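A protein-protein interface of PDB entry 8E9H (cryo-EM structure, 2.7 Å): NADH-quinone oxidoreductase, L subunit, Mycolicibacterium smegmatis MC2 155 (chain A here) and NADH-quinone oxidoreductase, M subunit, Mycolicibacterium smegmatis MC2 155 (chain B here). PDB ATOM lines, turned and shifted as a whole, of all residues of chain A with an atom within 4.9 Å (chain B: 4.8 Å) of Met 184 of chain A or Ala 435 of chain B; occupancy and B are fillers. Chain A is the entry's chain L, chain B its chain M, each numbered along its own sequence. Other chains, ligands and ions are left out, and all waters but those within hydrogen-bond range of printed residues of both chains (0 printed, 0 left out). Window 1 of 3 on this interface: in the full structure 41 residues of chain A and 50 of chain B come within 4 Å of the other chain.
Printed residues of chain A that touch a printed residue of chain B: Arg 180, Val 181, Met 184 and Ile 188.
Hydrophobic or aromatic side chains of chain A that line the printed part of chain B: Val 181, Met 184 and Ile 188.
Along chain A the printed residues that touch a printed residue of chain B span positions 180 to 188.
Of the 10 printed residues of chain B, 4 touch a printed residue of chain A.
Printed residues of chain B that touch a printed residue of chain A: Ala 435, Thr 436, Leu 438 and Val 439.
Hydrophobic or aromatic side chains of chain B that line the printed part of chain A: Ala 435, Leu 438 and Val 439.
Among the printed residues, 7 pairs touch across the chains.
Among the printed residues, no Asp or Glu carboxylate lies within 4 Å of a Lys or Arg side-chain nitrogen of the other chain.
Of the printed residues of chain B, Arg 180 of chain A touches Leu 438 (2.8 Å) and Val 439 (3.7 Å).
Printed residues of chain B within 4 Å of Val 181 of chain A: Val 439 (3.7 Å).
Of chain B, only Ala 435, Thr 436 and Val 439 come within 4 Å of Met 184 of chain A.
Of the printed residues of chain B, Ile 188 of chain A touches Ala 435 (3.5 Å).
Ala 435 of chain B touches just these residues of chain A: Met 184 (3.6 Å) and Ile 188 (3.5 Å).
Of the printed residues of chain A, Thr 436 of chain B touches Met 184 (3.6 Å).
Of the printed residues of chain A, Val 439 of chain B touches Arg 180 (3.7 Å), Val 181 (3.7 Å) and Met 184 (3.6 Å).
The nearest residue of chain B that does not touch Met 184 of chain A is Leu 438 of chain B (4.6 Å).
The nearest printed residue of chain A that does not touch Ala 435 of chain B is Ala 187 of chain A (5.7 Å).
CG of Arg 180 of chain A touches CA of Val 439 of chain B (3.7 Å).
Val 439 of chain B touches Val 181 of chain A.
Thr 436 of chain B touches Met 184 of chain A (CA to SD, 3.6 Å).
Val 439 of chain B touches Met 184 of chain A (CG2 to SD, 3.6 Å).
CB of Ala 435 of chain B touches CD1 of Ile 188 of chain A, 3.5 Å away.
The backbone carbonyl oxygen of Leu 438 of chain B sits at hydrogen-bond distance from the guanidinium group of Arg 180 of chain A.
SD of Met 184 of chain A lies close to O of Ala 435 of chain B.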
ATOM      1  N   TYR A 145     -28.104 -31.354  18.940  1.00  0.00           N
ATOM      2  CA  TYR A 145     -27.521 -30.025  19.072  1.00  0.00           C
ATOM      3  C   TYR A 145     -26.196 -30.076  19.813  1.00  0.00           C
ATOM      4  O   TYR A 145     -25.275 -29.309  19.513  1.00  0.00           O
ATOM      5  CB  TYR A 145     -28.490 -29.094  19.795  1.00  0.00           C
ATOM      6  CG  TYR A 145     -28.173 -27.637  19.589  1.00  0.00           C
ATOM      7  CD1 TYR A 145     -28.573 -26.976  18.441  1.00  0.00           C
ATOM      8  CD2 TYR A 145     -27.459 -26.926  20.538  1.00  0.00           C
ATOM      9  CE1 TYR A 145     -28.281 -25.647  18.248  1.00  0.00           C
ATOM     10  CE2 TYR A 145     -27.161 -25.595  20.353  1.00  0.00           C
ATOM     11  CZ  TYR A 145     -27.573 -24.960  19.208  1.00  0.00           C
ATOM     12  OH  TYR A 145     -27.276 -23.631  19.023  1.00  0.00           O
ATOM     13  N   ARG A 180     -22.477 -21.013  13.924  1.00  0.00           N
ATOM     14  CA  ARG A 180     -23.274 -20.649  15.085  1.00  0.00           C
ATOM     15  C   ARG A 180     -24.562 -19.962  14.671  1.00  0.00           C
ATOM     16  O   ARG A 180     -25.568 -20.073  15.368  1.00  0.00           O
ATOM     17  CB  ARG A 180     -22.462 -19.753  16.019  1.00  0.00           C
ATOM     18  CG  ARG A 180     -23.258 -19.159  17.173  1.00  0.00           C
ATOM     19  CD  ARG A 180     -23.994 -20.218  17.979  1.00  0.00           C
ATOM     20  NE  ARG A 180     -23.084 -21.047  18.760  1.00  0.00           N
ATOM     21  CZ  ARG A 180     -22.787 -20.847  20.036  1.00  0.00           C
ATOM     22  NH1 ARG A 180     -23.292 -19.831  20.717  1.00  0.00           N
ATOM     23  NH2 ARG A 180     -21.960 -21.689  20.647  1.00  0.00           N
ATOM     24  N   VAL A 181     -24.555 -19.246  13.550  1.00  0.00           N
ATOM     25  CA  VAL A 181     -25.818 -18.766  12.991  1.00  0.00           C
ATOM     26  C   VAL A 181     -26.699 -19.954  12.621  1.00  0.00           C
ATOM     27  O   VAL A 181     -27.906 -19.983  12.904  1.00  0.00           O
ATOM     28  CB  VAL A 181     -25.562 -17.856  11.778  1.00  0.00           C
ATOM     29  CG1 VAL A 181     -26.868 -17.526  11.085  1.00  0.00           C
ATOM     30  CG2 VAL A 181     -24.857 -16.587  12.213  1.00  0.00           C
ATOM     31  N   GLY A 182     -26.099 -20.956  11.984  1.00  0.00           N
ATOM     32  CA  GLY A 182     -26.840 -22.176  11.703  1.00  0.00           C
ATOM     33  C   GLY A 182     -27.358 -22.840  12.966  1.00  0.00           C
ATOM     34  O   GLY A 182     -28.501 -23.299  13.021  1.00  0.00           O
ATOM     35  N   ASP A 183     -26.518 -22.900  13.998  1.00  0.00           N
ATOM     36  CA  ASP A 183     -26.929 -23.479  15.268  1.00  0.00           C
ATOM     37  C   ASP A 183     -28.027 -22.656  15.920  1.00  0.00           C
ATOM     38  O   ASP A 183     -28.876 -23.208  16.618  1.00  0.00           O
ATOM     39  CB  ASP A 183     -25.730 -23.597  16.206  1.00  0.00           C
ATOM     40  N   MET A 184     -28.024 -21.341  15.716  1.00  0.00           N
ATOM     41  CA  MET A 184     -29.121 -20.512  16.195  1.00  0.00           C
ATOM     42  C   MET A 184     -30.418 -20.900  15.508  1.00  0.00           C
ATOM     43  O   MET A 184     -31.463 -21.038  16.154  1.00  0.00           O
ATOM     44  CB  MET A 184     -28.809 -19.039  15.944  1.00  0.00           C
ATOM     45  CG  MET A 184     -29.872 -18.090  16.455  1.00  0.00           C
ATOM     46  SD  MET A 184     -29.442 -16.370  16.154  1.00  0.00           S
ATOM     47  CE  MET A 184     -29.662 -16.269  14.382  1.00  0.00           C
ATOM     48  N   GLY A 185     -30.369 -21.078  14.190  1.00  0.00           N
ATOM     49  CA  GLY A 185     -31.550 -21.553  13.487  1.00  0.00           C
ATOM     50  C   GLY A 185     -32.035 -22.882  14.032  1.00  0.00           C
ATOM     51  O   GLY A 185     -33.227 -23.078  14.282  1.00  0.00           O
ATOM     52  N   LEU A 186     -31.103 -23.809  14.247  1.00  0.00           N
ATOM     53  CA  LEU A 186     -31.473 -25.118  14.777  1.00  0.00           C
ATOM     54  C   LEU A 186     -32.033 -25.001  16.190  1.00  0.00           C
ATOM     55  O   LEU A 186     -32.919 -25.767  16.585  1.00  0.00           O
ATOM     56  CB  LEU A 186     -30.262 -26.046  14.750  1.00  0.00           C
ATOM     57  CG  LEU A 186     -30.416 -27.388  15.465  1.00  0.00           C
ATOM     58  CD1 LEU A 186     -31.603 -28.153  14.913  1.00  0.00           C
ATOM     59  CD2 LEU A 186     -29.144 -28.201  15.325  1.00  0.00           C
ATOM     60  N   ALA A 187     -31.514 -24.058  16.976  1.00  0.00           N
ATOM     61  CA  ALA A 187     -32.022 -23.848  18.324  1.00  0.00           C
ATOM     62  C   ALA A 187     -33.448 -23.327  18.293  1.00  0.00           C
ATOM     63  O   ALA A 187     -34.293 -23.768  19.076  1.00  0.00           O
ATOM     64  CB  ALA A 187     -31.116 -22.882  19.083  1.00  0.00           C
ATOM     65  N   ILE A 188     -33.735 -22.381  17.398  1.00  0.00           N
ATOM     66  CA  ILE A 188     -35.118 -21.942  17.232  1.00  0.00           C
ATOM     67  C   ILE A 188     -35.986 -23.117  16.818  1.00  0.00           C
ATOM     68  O   ILE A 188     -37.140 -23.239  17.246  1.00  0.00           O
ATOM     69  CB  ILE A 188     -35.223 -20.788  16.217  1.00  0.00           C
ATOM     70  CG1 ILE A 188     -34.210 -19.681  16.506  1.00  0.00           C
ATOM     71  CG2 ILE A 188     -36.626 -20.209  16.231  1.00  0.00           C
ATOM     72  CD1 ILE A 188     -34.129 -19.263  17.945  1.00  0.00           C
ATOM     73  N   LEU B 420     -34.082 -20.273  27.208  1.00  0.00           N
ATOM     74  CA  LEU B 420     -34.665 -19.967  25.908  1.00  0.00           C
ATOM     75  C   LEU B 420     -35.930 -20.777  25.688  1.00  0.00           C
ATOM     76  O   LEU B 420     -36.979 -20.231  25.325  1.00  0.00           O
ATOM     77  CB  LEU B 420     -33.651 -20.241  24.800  1.00  0.00           C
ATOM     78  CG  LEU B 420     -32.546 -19.198  24.644  1.00  0.00           C
ATOM     79  CD1 LEU B 420     -31.515 -19.668  23.636  1.00  0.00           C
ATOM     80  CD2 LEU B 420     -33.122 -17.854  24.235  1.00  0.00           C
ATOM     81  N   ALA B 431     -37.911 -14.723  22.819  1.00  0.00           N
ATOM     82  CA  ALA B 431     -37.015 -15.872  22.809  1.00  0.00           C
ATOM     83  C   ALA B 431     -36.052 -15.805  21.633  1.00  0.00           C
ATOM     84  O   ALA B 431     -34.852 -16.044  21.793  1.00  0.00           O
ATOM     85  CB  ALA B 431     -37.824 -17.167  22.768  1.00  0.00           C
ATOM     86  N   VAL B 432     -36.554 -15.475  20.442  1.00  0.00           N
ATOM     87  CA  VAL B 432     -35.674 -15.367  19.277  1.00  0.00           C
ATOM     88  C   VAL B 432     -34.689 -14.217  19.462  1.00  0.00           C
ATOM     89  O   VAL B 432     -33.491 -14.330  19.151  1.00  0.00           O
ATOM     90  CB  VAL B 432     -36.507 -15.192  17.996  1.00  0.00           C
ATOM     91  CG1 VAL B 432     -35.604 -14.889  16.815  1.00  0.00           C
ATOM     92  CG2 VAL B 432     -37.335 -16.434  17.734  1.00  0.00           C
ATOM     93  N   PHE B 433     -35.186 -13.084  19.958  1.00  0.00           N
ATOM     94  CA  PHE B 433     -34.328 -11.923  20.153  1.00  0.00           C
ATOM     95  C   PHE B 433     -33.181 -12.263  21.091  1.00  0.00           C
ATOM     96  O   PHE B 433     -32.037 -11.850  20.873  1.00  0.00           O
ATOM     97  CB  PHE B 433     -35.159 -10.762  20.696  1.00  0.00           C
ATOM     98  CG  PHE B 433     -34.403  -9.475  20.818  1.00  0.00           C
ATOM     99  CD1 PHE B 433     -33.876  -8.859  19.699  1.00  0.00           C
ATOM    100  CD2 PHE B 433     -34.230  -8.874  22.051  1.00  0.00           C
ATOM    101  CE1 PHE B 433     -33.184  -7.670  19.810  1.00  0.00           C
ATOM    102  CE2 PHE B 433     -33.540  -7.686  22.166  1.00  0.00           C
ATOM    103  CZ  PHE B 433     -33.016  -7.084  21.045  1.00  0.00           C
ATOM    104  N   ALA B 434     -33.473 -13.025  22.147  1.00  0.00           N
ATOM    105  CA  ALA B 434     -32.420 -13.482  23.044  1.00  0.00           C
ATOM    106  C   ALA B 434     -31.502 -14.480  22.351  1.00  0.00           C
ATOM    107  O   ALA B 434     -30.279 -14.426  22.515  1.00  0.00           O
ATOM    108  CB  ALA B 434     -33.034 -14.102  24.295  1.00  0.00           C
ATOM    109  N   ALA B 435     -32.072 -15.395  21.566  1.00  0.00           N
ATOM    110  CA  ALA B 435     -31.261 -16.401  20.895  1.00  0.00           C
ATOM    111  C   ALA B 435     -30.219 -15.774  19.987  1.00  0.00           C
ATOM    112  O   ALA B 435     -29.172 -16.382  19.749  1.00  0.00           O
ATOM    113  CB  ALA B 435     -32.154 -17.342  20.090  1.00  0.00           C
ATOM    114  N   THR B 436     -30.482 -14.571  19.479  1.00  0.00           N
ATOM    115  CA  THR B 436     -29.445 -13.869  18.719  1.00  0.00           C
ATOM    116  C   THR B 436     -28.161 -13.734  19.532  1.00  0.00           C
ATOM    117  O   THR B 436     -27.055 -13.671  18.970  1.00  0.00           O
ATOM    118  CB  THR B 436     -29.936 -12.488  18.293  1.00  0.00           C
ATOM    119  OG1 THR B 436     -30.166 -11.683  19.456  1.00  0.00           O
ATOM    120  CG2 THR B 436     -31.221 -12.599  17.491  1.00  0.00           C
ATOM    121  N   ALA B 437     -28.283 -13.681  20.856  1.00  0.00           N
ATOM    122  CA  ALA B 437     -27.097 -13.621  21.694  1.00  0.00           C
ATOM    123  C   ALA B 437     -26.234 -14.862  21.553  1.00  0.00           C
ATOM    124  O   ALA B 437     -25.052 -14.809  21.888  1.00  0.00           O
ATOM    125  CB  ALA B 437     -27.492 -13.425  23.151  1.00  0.00           C
ATOM    126  N   LEU B 438     -26.779 -15.972  21.055  1.00  0.00           N
ATOM    127  CA  LEU B 438     -25.929 -17.128  20.789  1.00  0.00           C
ATOM    128  C   LEU B 438     -24.869 -16.794  19.749  1.00  0.00           C
ATOM    129  O   LEU B 438     -23.699 -17.166  19.901  1.00  0.00           O
ATOM    130  CB  LEU B 438     -26.773 -18.312  20.326  1.00  0.00           C
ATOM    131  CG  LEU B 438     -27.706 -18.920  21.370  1.00  0.00           C
ATOM    132  CD1 LEU B 438     -28.702 -19.847  20.702  1.00  0.00           C
ATOM    133  CD2 LEU B 438     -26.911 -19.663  22.430  1.00  0.00           C
ATOM    134  N   VAL B 439     -25.259 -16.100  18.681  1.00  0.00           N
ATOM    135  CA  VAL B 439     -24.289 -15.664  17.683  1.00  0.00           C
ATOM    136  C   VAL B 439     -23.413 -14.556  18.248  1.00  0.00           C
ATOM    137  O   VAL B 439     -22.196 -14.520  18.020  1.00  0.00           O
ATOM    138  CB  VAL B 439     -25.010 -15.207  16.403  1.00  0.00           C
ATOM    139  CG1 VAL B 439     -24.004 -14.754  15.363  1.00  0.00           C
ATOM    140  CG2 VAL B 439     -25.882 -16.322  15.859  1.00  0.00           C
